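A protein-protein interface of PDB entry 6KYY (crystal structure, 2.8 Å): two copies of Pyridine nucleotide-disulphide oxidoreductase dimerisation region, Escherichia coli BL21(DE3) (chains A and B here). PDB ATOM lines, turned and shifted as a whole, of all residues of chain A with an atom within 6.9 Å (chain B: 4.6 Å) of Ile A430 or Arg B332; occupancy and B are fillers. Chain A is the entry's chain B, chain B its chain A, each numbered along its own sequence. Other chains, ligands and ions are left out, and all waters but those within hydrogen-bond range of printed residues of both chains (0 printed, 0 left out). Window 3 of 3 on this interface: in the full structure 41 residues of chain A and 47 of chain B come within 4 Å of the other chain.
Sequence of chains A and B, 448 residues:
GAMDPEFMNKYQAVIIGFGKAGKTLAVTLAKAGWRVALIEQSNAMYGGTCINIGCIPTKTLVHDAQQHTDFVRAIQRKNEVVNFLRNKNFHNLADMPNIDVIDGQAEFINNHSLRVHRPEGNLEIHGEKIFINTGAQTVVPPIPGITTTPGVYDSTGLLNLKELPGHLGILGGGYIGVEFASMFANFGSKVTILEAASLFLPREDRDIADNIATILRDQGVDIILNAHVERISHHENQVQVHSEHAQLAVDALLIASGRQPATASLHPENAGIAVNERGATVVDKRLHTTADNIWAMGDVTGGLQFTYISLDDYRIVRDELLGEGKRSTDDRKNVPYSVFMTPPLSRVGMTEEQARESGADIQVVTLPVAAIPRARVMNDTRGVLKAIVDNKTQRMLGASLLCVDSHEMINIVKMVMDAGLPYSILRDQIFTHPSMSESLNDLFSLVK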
ATOM      1  N   ILE A 425      -1.427 -19.146  -7.660  1.00  0.00           N
ATOM      2  CA  ILE A 425      -0.919 -17.970  -8.362  1.00  0.00           C
ATOM      3  C   ILE A 425       0.530 -17.703  -7.970  1.00  0.00           C
ATOM      4  O   ILE A 425       1.392 -17.470  -8.826  1.00  0.00           O
ATOM      5  CB  ILE A 425      -1.818 -16.751  -8.087  1.00  0.00           C
ATOM      6  CG1 ILE A 425      -2.968 -16.702  -9.093  1.00  0.00           C
ATOM      7  CG2 ILE A 425      -1.015 -15.459  -8.144  1.00  0.00           C
ATOM      8  CD1 ILE A 425      -2.526 -16.404 -10.510  1.00  0.00           C
ATOM      9  N   LEU A 426       0.822 -17.744  -6.669  1.00  0.00           N
ATOM     10  CA  LEU A 426       2.180 -17.497  -6.203  1.00  0.00           C
ATOM     11  C   LEU A 426       3.088 -18.707  -6.373  1.00  0.00           C
ATOM     12  O   LEU A 426       4.313 -18.548  -6.391  1.00  0.00           O
ATOM     13  CB  LEU A 426       2.159 -17.057  -4.738  1.00  0.00           C
ATOM     14  CG  LEU A 426       1.356 -15.782  -4.464  1.00  0.00           C
ATOM     15  CD1 LEU A 426       1.317 -15.465  -2.977  1.00  0.00           C
ATOM     16  CD2 LEU A 426       1.924 -14.612  -5.252  1.00  0.00           C
ATOM     17  N   ASP A 428       3.270 -20.478  -9.105  1.00  0.00           N
ATOM     18  CA  ASP A 428       3.657 -20.589 -10.503  1.00  0.00           C
ATOM     19  C   ASP A 428       4.079 -19.273 -11.140  1.00  0.00           C
ATOM     20  O   ASP A 428       4.378 -19.257 -12.340  1.00  0.00           O
ATOM     21  CB  ASP A 428       2.509 -21.196 -11.323  1.00  0.00           C
ATOM     22  CG  ASP A 428       2.237 -22.640 -10.962  1.00  0.00           C
ATOM     23  OD1 ASP A 428       3.196 -23.353 -10.594  1.00  0.00           O
ATOM     24  OD2 ASP A 428       1.066 -23.064 -11.043  1.00  0.00           O
ATOM     25  N   GLN A 429       4.122 -18.178 -10.386  1.00  0.00           N
ATOM     26  CA  GLN A 429       4.457 -16.890 -10.974  1.00  0.00           C
ATOM     27  C   GLN A 429       5.939 -16.816 -11.319  1.00  0.00           C
ATOM     28  O   GLN A 429       6.794 -17.381 -10.630  1.00  0.00           O
ATOM     29  CB  GLN A 429       4.086 -15.754 -10.023  1.00  0.00           C
ATOM     30  CG  GLN A 429       4.115 -14.376 -10.664  1.00  0.00           C
ATOM     31  CD  GLN A 429       3.366 -13.345  -9.852  1.00  0.00           C
ATOM     32  OE1 GLN A 429       2.149 -13.426  -9.700  1.00  0.00           O
ATOM     33  NE2 GLN A 429       4.090 -12.365  -9.323  1.00  0.00           N
ATOM     34  N   ILE A 430       6.239 -16.108 -12.405  1.00  0.00           N
ATOM     35  CA  ILE A 430       7.608 -15.933 -12.876  1.00  0.00           C
ATOM     36  C   ILE A 430       8.176 -14.704 -12.173  1.00  0.00           C
ATOM     37  O   ILE A 430       7.993 -13.571 -12.620  1.00  0.00           O
ATOM     38  CB  ILE A 430       7.669 -15.800 -14.398  1.00  0.00           C
ATOM     39  CG1 ILE A 430       6.944 -16.976 -15.060  1.00  0.00           C
ATOM     40  CG2 ILE A 430       9.111 -15.720 -14.863  1.00  0.00           C
ATOM     41  CD1 ILE A 430       7.310 -17.193 -16.507  1.00  0.00           C
ATOM     42  N   PHE A 431       8.877 -14.937 -11.067  1.00  0.00           N
ATOM     43  CA  PHE A 431       9.434 -13.870 -10.251  1.00  0.00           C
ATOM     44  C   PHE A 431      10.843 -13.511 -10.710  1.00  0.00           C
ATOM     45  O   PHE A 431      11.506 -14.268 -11.422  1.00  0.00           O
ATOM     46  CB  PHE A 431       9.465 -14.280  -8.779  1.00  0.00           C
ATOM     47  CG  PHE A 431       8.122 -14.251  -8.106  1.00  0.00           C
ATOM     48  CD1 PHE A 431       7.551 -13.049  -7.718  1.00  0.00           C
ATOM     49  CD2 PHE A 431       7.435 -15.426  -7.852  1.00  0.00           C
ATOM     50  CE1 PHE A 431       6.318 -13.020  -7.095  1.00  0.00           C
ATOM     51  CE2 PHE A 431       6.200 -15.404  -7.228  1.00  0.00           C
ATOM     52  CZ  PHE A 431       5.640 -14.199  -6.851  1.00  0.00           C
ATOM     53  N   THR A 432      11.299 -12.337 -10.279  1.00  0.00           N
ATOM     54  CA  THR A 432      12.662 -11.912 -10.550  1.00  0.00           C
ATOM     55  C   THR A 432      13.651 -12.778  -9.770  1.00  0.00           C
ATOM     56  O   THR A 432      13.320 -13.372  -8.741  1.00  0.00           O
ATOM     57  CB  THR A 432      12.847 -10.437 -10.193  1.00  0.00           C
ATOM     58  OG1 THR A 432      12.095 -10.134  -9.011  1.00  0.00           O
ATOM     59  CG2 THR A 432      12.363  -9.552 -11.332  1.00  0.00           C
ATOM     60  N   GLU A 438      10.765 -14.482  -4.970  1.00  0.00           N
ATOM     61  CA  GLU A 438      10.715 -15.703  -5.765  1.00  0.00           C
ATOM     62  C   GLU A 438      10.591 -16.950  -4.904  1.00  0.00           C
ATOM     63  O   GLU A 438      10.097 -17.974  -5.387  1.00  0.00           O
ATOM     64  CB  GLU A 438      11.958 -15.812  -6.648  1.00  0.00           C
ATOM     65  CG  GLU A 438      13.227 -16.108  -5.873  1.00  0.00           C
ATOM     66  CD  GLU A 438      14.319 -16.693  -6.735  1.00  0.00           C
ATOM     67  OE1 GLU A 438      14.004 -17.508  -7.627  1.00  0.00           O
ATOM     68  OE2 GLU A 438      15.497 -16.343  -6.519  1.00  0.00           O
ATOM     69  N   ASN A 441       7.636 -19.163  -4.867  1.00  0.00           N
ATOM     70  CA  ASN A 441       7.533 -20.317  -5.756  1.00  0.00           C
ATOM     71  C   ASN A 441       7.829 -21.606  -5.001  1.00  0.00           C
ATOM     72  O   ASN A 441       7.105 -22.599  -5.129  1.00  0.00           O
ATOM     73  CB  ASN A 441       8.494 -20.164  -6.937  1.00  0.00           C
ATOM     74  CG  ASN A 441       7.979 -19.209  -7.993  1.00  0.00           C
ATOM     75  OD1 ASN A 441       6.787 -18.910  -8.049  1.00  0.00           O
ATOM     76  ND2 ASN A 441       8.880 -18.724  -8.841  1.00  0.00           N
ATOM     77  N   TYR B 308      14.511 -17.890 -14.047  1.00  0.00           N
ATOM     78  CA  TYR B 308      13.085 -18.107 -13.819  1.00  0.00           C
ATOM     79  C   TYR B 308      12.380 -18.605 -15.074  1.00  0.00           C
ATOM     80  O   TYR B 308      11.429 -19.389 -14.976  1.00  0.00           O
ATOM     81  CB  TYR B 308      12.420 -16.825 -13.312  1.00  0.00           C
ATOM     82  CG  TYR B 308      12.992 -15.536 -13.865  1.00  0.00           C
ATOM     83  CD1 TYR B 308      14.041 -14.891 -13.226  1.00  0.00           C
ATOM     84  CD2 TYR B 308      12.470 -14.953 -15.011  1.00  0.00           C
ATOM     85  CE1 TYR B 308      14.564 -13.711 -13.717  1.00  0.00           C
ATOM     86  CE2 TYR B 308      12.983 -13.769 -15.508  1.00  0.00           C
ATOM     87  CZ  TYR B 308      14.032 -13.154 -14.857  1.00  0.00           C
ATOM     88  OH  TYR B 308      14.551 -11.979 -15.348  1.00  0.00           O
ATOM     89  N   ILE B 309      12.823 -18.165 -16.254  1.00  0.00           N
ATOM     90  CA  ILE B 309      12.220 -18.646 -17.493  1.00  0.00           C
ATOM     91  C   ILE B 309      12.515 -20.128 -17.688  1.00  0.00           C
ATOM     92  O   ILE B 309      11.661 -20.889 -18.158  1.00  0.00           O
ATOM     93  CB  ILE B 309      12.707 -17.800 -18.684  1.00  0.00           C
ATOM     94  CG1 ILE B 309      12.139 -16.384 -18.589  1.00  0.00           C
ATOM     95  CG2 ILE B 309      12.298 -18.436 -20.003  1.00  0.00           C
ATOM     96  CD1 ILE B 309      10.630 -16.344 -18.496  1.00  0.00           C
ATOM     97  N   ASP B 312      10.187 -22.072 -15.543  1.00  0.00           N
ATOM     98  CA  ASP B 312       8.882 -22.174 -16.183  1.00  0.00           C
ATOM     99  C   ASP B 312       8.916 -23.133 -17.365  1.00  0.00           C
ATOM    100  O   ASP B 312       7.885 -23.722 -17.712  1.00  0.00           O
ATOM    101  CB  ASP B 312       8.397 -20.797 -16.630  1.00  0.00           C
ATOM    102  CG  ASP B 312       6.920 -20.790 -16.974  1.00  0.00           C
ATOM    103  OD1 ASP B 312       6.580 -20.464 -18.131  1.00  0.00           O
ATOM    104  OD2 ASP B 312       6.101 -21.119 -16.089  1.00  0.00           O
ATOM    105  N   ASP B 313      10.080 -23.298 -18.000  1.00  0.00           N
ATOM    106  CA  ASP B 313      10.221 -24.348 -19.001  1.00  0.00           C
ATOM    107  C   ASP B 313      10.001 -25.723 -18.384  1.00  0.00           C
ATOM    108  O   ASP B 313       9.466 -26.622 -19.042  1.00  0.00           O
ATOM    109  CB  ASP B 313      11.600 -24.271 -19.659  1.00  0.00           C
ATOM    110  CG  ASP B 313      11.641 -23.300 -20.822  1.00  0.00           C
ATOM    111  OD1 ASP B 313      10.561 -22.902 -21.306  1.00  0.00           O
ATOM    112  OD2 ASP B 313      12.755 -22.937 -21.254  1.00  0.00           O
ATOM    113  N   ARG B 315       7.951 -26.112 -15.813  1.00  0.00           N
ATOM    114  CA  ARG B 315       6.507 -26.115 -15.610  1.00  0.00           C
ATOM    115  C   ARG B 315       5.776 -26.532 -16.880  1.00  0.00           C
ATOM    116  O   ARG B 315       4.810 -27.303 -16.827  1.00  0.00           O
ATOM    117  CB  ARG B 315       6.038 -24.730 -15.157  1.00  0.00           C
ATOM    118  CG  ARG B 315       6.466 -24.340 -13.744  1.00  0.00           C
ATOM    119  CD  ARG B 315       5.755 -23.071 -13.294  1.00  0.00           C
ATOM    120  NE  ARG B 315       6.570 -21.878 -13.502  1.00  0.00           N
ATOM    121  CZ  ARG B 315       7.184 -21.214 -12.528  1.00  0.00           C
ATOM    122  NH1 ARG B 315       7.078 -21.631 -11.273  1.00  0.00           N
ATOM    123  NH2 ARG B 315       7.906 -20.137 -12.804  1.00  0.00           N
ATOM    124  N   ILE B 316       6.225 -26.033 -18.036  1.00  0.00           N
ATOM    125  CA  ILE B 316       5.576 -26.382 -19.296  1.00  0.00           C
ATOM    126  C   ILE B 316       5.767 -27.863 -19.598  1.00  0.00           C
ATOM    127  O   ILE B 316       4.841 -28.546 -20.054  1.00  0.00           O
ATOM    128  CB  ILE B 316       6.115 -25.502 -20.443  1.00  0.00           C
ATOM    129  CG1 ILE B 316       5.863 -24.023 -20.147  1.00  0.00           C
ATOM    130  CG2 ILE B 316       5.501 -25.906 -21.776  1.00  0.00           C
ATOM    131  CD1 ILE B 316       6.726 -23.063 -20.956  1.00  0.00           C
ATOM    132  N   ARG B 327      -0.252 -26.302 -20.471  1.00  0.00           N
ATOM    133  CA  ARG B 327       0.847 -25.357 -20.319  1.00  0.00           C
ATOM    134  C   ARG B 327       1.589 -25.150 -21.643  1.00  0.00           C
ATOM    135  O   ARG B 327       1.885 -26.108 -22.354  1.00  0.00           O
ATOM    136  CB  ARG B 327       1.800 -25.851 -19.225  1.00  0.00           C
ATOM    137  CG  ARG B 327       1.333 -25.405 -17.835  1.00  0.00           C
ATOM    138  CD  ARG B 327       1.228 -23.876 -17.740  1.00  0.00           C
ATOM    139  NE  ARG B 327       2.451 -23.232 -18.208  1.00  0.00           N
ATOM    140  CZ  ARG B 327       2.636 -21.916 -18.214  1.00  0.00           C
ATOM    141  NH1 ARG B 327       1.691 -21.104 -17.769  1.00  0.00           N
ATOM    142  NH2 ARG B 327       3.763 -21.398 -18.665  1.00  0.00           N
ATOM    143  N   THR B 329       4.209 -22.106 -24.051  1.00  0.00           N
ATOM    144  CA  THR B 329       4.997 -20.890 -24.014  1.00  0.00           C
ATOM    145  C   THR B 329       4.181 -19.678 -24.437  1.00  0.00           C
ATOM    146  O   THR B 329       4.680 -18.552 -24.343  1.00  0.00           O
ATOM    147  CB  THR B 329       6.237 -21.042 -24.891  1.00  0.00           C
ATOM    148  OG1 THR B 329       7.264 -20.181 -24.393  1.00  0.00           O
ATOM    149  CG2 THR B 329       5.935 -20.672 -26.340  1.00  0.00           C
ATOM    150  N   ASP B 330       2.939 -19.882 -24.887  1.00  0.00           N
ATOM    151  CA  ASP B 330       2.005 -18.791 -25.135  1.00  0.00           C
ATOM    152  C   ASP B 330       1.242 -18.378 -23.878  1.00  0.00           C
ATOM    153  O   ASP B 330       0.167 -17.775 -23.981  1.00  0.00           O
ATOM    154  CB  ASP B 330       1.018 -19.162 -26.245  1.00  0.00           C
ATOM    155  CG  ASP B 330       1.693 -19.348 -27.587  1.00  0.00           C
ATOM    156  OD1 ASP B 330       1.047 -19.892 -28.509  1.00  0.00           O
ATOM    157  OD2 ASP B 330       2.870 -18.955 -27.719  1.00  0.00           O
ATOM    158  N   ASP B 331       1.776 -18.697 -22.699  1.00  0.00           N
ATOM    159  CA  ASP B 331       1.197 -18.289 -21.429  1.00  0.00           C
ATOM    160  C   ASP B 331       1.971 -17.171 -20.751  1.00  0.00           C
ATOM    161  O   ASP B 331       1.414 -16.499 -19.877  1.00  0.00           O
ATOM    162  CB  ASP B 331       1.132 -19.484 -20.466  1.00  0.00           C
ATOM    163  CG  ASP B 331      -0.213 -20.181 -20.482  1.00  0.00           C
ATOM    164  OD1 ASP B 331      -1.189 -19.608 -19.952  1.00  0.00           O
ATOM    165  OD2 ASP B 331      -0.291 -21.309 -21.012  1.00  0.00           O
ATOM    166  N   ARG B 332       3.227 -16.955 -21.135  1.00  0.00           N
ATOM    167  CA  ARG B 332       4.134 -16.057 -20.422  1.00  0.00           C
ATOM    168  C   ARG B 332       3.861 -14.618 -20.834  1.00  0.00           C
ATOM    169  O   ARG B 332       4.455 -14.089 -21.775  1.00  0.00           O
ATOM    170  CB  ARG B 332       5.583 -16.439 -20.691  1.00  0.00           C
ATOM    171  CG  ARG B 332       5.894 -17.898 -20.433  1.00  0.00           C
ATOM    172  CD  ARG B 332       7.359 -18.084 -20.089  1.00  0.00           C
ATOM    173  NE  ARG B 332       8.097 -18.726 -21.171  1.00  0.00           N
ATOM    174  CZ  ARG B 332       9.000 -19.684 -20.991  1.00  0.00           C
ATOM    175  NH1 ARG B 332       9.276 -20.111 -19.767  1.00  0.00           N
ATOM    176  NH2 ARG B 332       9.626 -20.213 -22.031  1.00  0.00           N
ATOM    177  N   LYS B 333       2.951 -13.974 -20.111  1.00  0.00           N
ATOM    178  CA  LYS B 333       2.728 -12.545 -20.244  1.00  0.00           C
ATOM    179  C   LYS B 333       3.603 -11.798 -19.247  1.00  0.00           C
ATOM    180  O   LYS B 333       3.728 -12.207 -18.089  1.00  0.00           O
ATOM    181  CB  LYS B 333       1.259 -12.196 -20.003  1.00  0.00           C
ATOM    182  CG  LYS B 333       0.411 -12.073 -21.260  1.00  0.00           C
ATOM    183  CD  LYS B 333      -1.042 -11.762 -20.913  1.00  0.00           C
ATOM    184  CE  LYS B 333      -1.152 -10.986 -19.604  1.00  0.00           C
ATOM    185  NZ  LYS B 333      -2.537 -10.518 -19.332  1.00  0.00           N
ATOM    186  N   ASN B 334       4.217 -10.708 -19.710  1.00  0.00           N
ATOM    187  CA  ASN B 334       4.941  -9.765 -18.857  1.00  0.00           C
ATOM    188  C   ASN B 334       6.052 -10.468 -18.067  1.00  0.00           C
ATOM    189  O   ASN B 334       5.999 -10.615 -16.845  1.00  0.00           O
ATOM    190  CB  ASN B 334       3.973  -9.041 -17.915  1.00  0.00           C
ATOM    191  CG  ASN B 334       2.846  -8.354 -18.657  1.00  0.00           C
ATOM    192  OD1 ASN B 334       1.741  -8.210 -18.135  1.00  0.00           O
ATOM    193  ND2 ASN B 334       3.121  -7.920 -19.882  1.00  0.00           N
ATOM    194  N   VAL B 335       7.067 -10.898 -18.809  1.00  0.00           N
ATOM    195  CA  VAL B 335       8.257 -11.483 -18.200  1.00  0.00           C
ATOM    196  C   VAL B 335       9.138 -10.344 -17.699  1.00  0.00           C
ATOM    197  O   VAL B 335       9.615  -9.531 -18.504  1.00  0.00           O
ATOM    198  CB  VAL B 335       9.013 -12.384 -19.190  1.00  0.00           C
ATOM    199  CG1 VAL B 335      10.420 -12.665 -18.683  1.00  0.00           C
ATOM    200  CG2 VAL B 335       8.251 -13.681 -19.411  1.00  0.00           C
ATOM    201  N   PRO B 336       9.369 -10.234 -16.394  1.00  0.00           N
ATOM    202  CA  PRO B 336      10.204  -9.153 -15.872  1.00  0.00           C
ATOM    203  C   PRO B 336      11.670  -9.553 -15.796  1.00  0.00           C
ATOM    204  O   PRO B 336      12.030 -10.731 -15.836  1.00  0.00           O
ATOM    205  CB  PRO B 336       9.627  -8.931 -14.468  1.00  0.00           C
ATOM    206  CG  PRO B 336       9.189 -10.303 -14.051  1.00  0.00           C
ATOM    207  CD  PRO B 336       8.832 -11.077 -15.312  1.00  0.00           C
ATOM    208  N   LYS B 414       4.112  -6.672 -12.114  1.00  0.00           N
ATOM    209  CA  LYS B 414       3.931  -7.754 -13.077  1.00  0.00           C
ATOM    210  C   LYS B 414       2.704  -8.595 -12.748  1.00  0.00           C
ATOM    211  O   LYS B 414       1.970  -9.016 -13.650  1.00  0.00           O
ATOM    212  CB  LYS B 414       5.183  -8.631 -13.120  1.00  0.00           C
ATOM    213  CG  LYS B 414       4.964  -9.984 -13.775  1.00  0.00           C
ATOM    214  CD  LYS B 414       5.848 -11.062 -13.164  1.00  0.00           C
ATOM    215  CE  LYS B 414       5.954 -10.930 -11.654  1.00  0.00           C
ATOM    216  NZ  LYS B 414       7.049 -11.777 -11.110  1.00  0.00           N
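The backbone carbonyl oxygen (O) of Ile A430 lies within hydrogen-bond range of the side-chain amino group (NZ) of Lys B414 (2.5 Å).
Hydrophobic or aromatic side chains of chain B that line the printed part of chain A: Tyr B308, Ile B309 and Pro B336. Hydrophobic or aromatic side chains of chain A within 4 Å of the printed part of chain B: Ile A430 and Phe A431. Among the printed residues, 11 pairs touch across the chains. Among the printed residues, no Asp or Glu carboxylate lies within 4 Å of a Lys or Arg side-chain nitrogen of the other chain.
No position is printed for both chains. Of the 11 pairs that touch across the chains among the printed residues, none has its exchanged pair printed and touching as well.
The side-chain carboxylate of Asp B312 is in salt-bridge range of the guanidinium group of Arg B315, 2.7 Å away. OH of Tyr B308 sits at hydrogen-bond distance from O of Pro B336 (2.9 Å). The side-chain carboxylate of Asp B313 lies within salt-bridge range of the guanidinium group of Arg B332, at 2.9 Å. The guanidinium group (NH1) of Arg B332 is in salt-bridge range of the side-chain carboxylate (OD1) of Asp B312 (3.2 Å). The guanidinium group (NH1) of Arg B332 is in hydrogen-bond range of the backbone carbonyl oxygen (O) of Ile B309 (3.0 Å). The backbone carbonyl oxygen (O) of Gln A429 lies close to the side-chain amide oxygen (OD1) of Asn A441 (3.0 Å).
Of the printed residues of chain B, Asp A428 touches Arg B315. Printed residues of chain A within 4 Å of Arg B315: Asp A428 and Gln A429. Of the printed residues of chain A, Arg B332 touches Ile A430 (3.7 Å). Lys B333 touches none of the printed residues of chain A. The nearest printed residue of chain B that does not touch Ile A430 is Arg B315 (4.001 Å).
Arg B315 touches Asp A428 (CZ to O, 3.4 Å). Gln A429 touches Arg B315 (O to NH2, 3.7 Å). Gln A429 touches Lys B414 (NE2 to CE, 3.3 Å). Ile A430 touches Tyr B308. Ile A430 touches Ile B309. CD1 of Ile A430 touches CG of Asp B312, 3.6 Å away. CD1 of Ile A430 touches CD of Arg B332, 3.7 Å away. Ile A430 touches Pro B336 (O to CG, 3.8 Å). Tyr B308 touches Phe A431 (CG to O, 3.1 Å). Lys B414 touches Phe A431 (NZ to CA, 3.3 Å).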
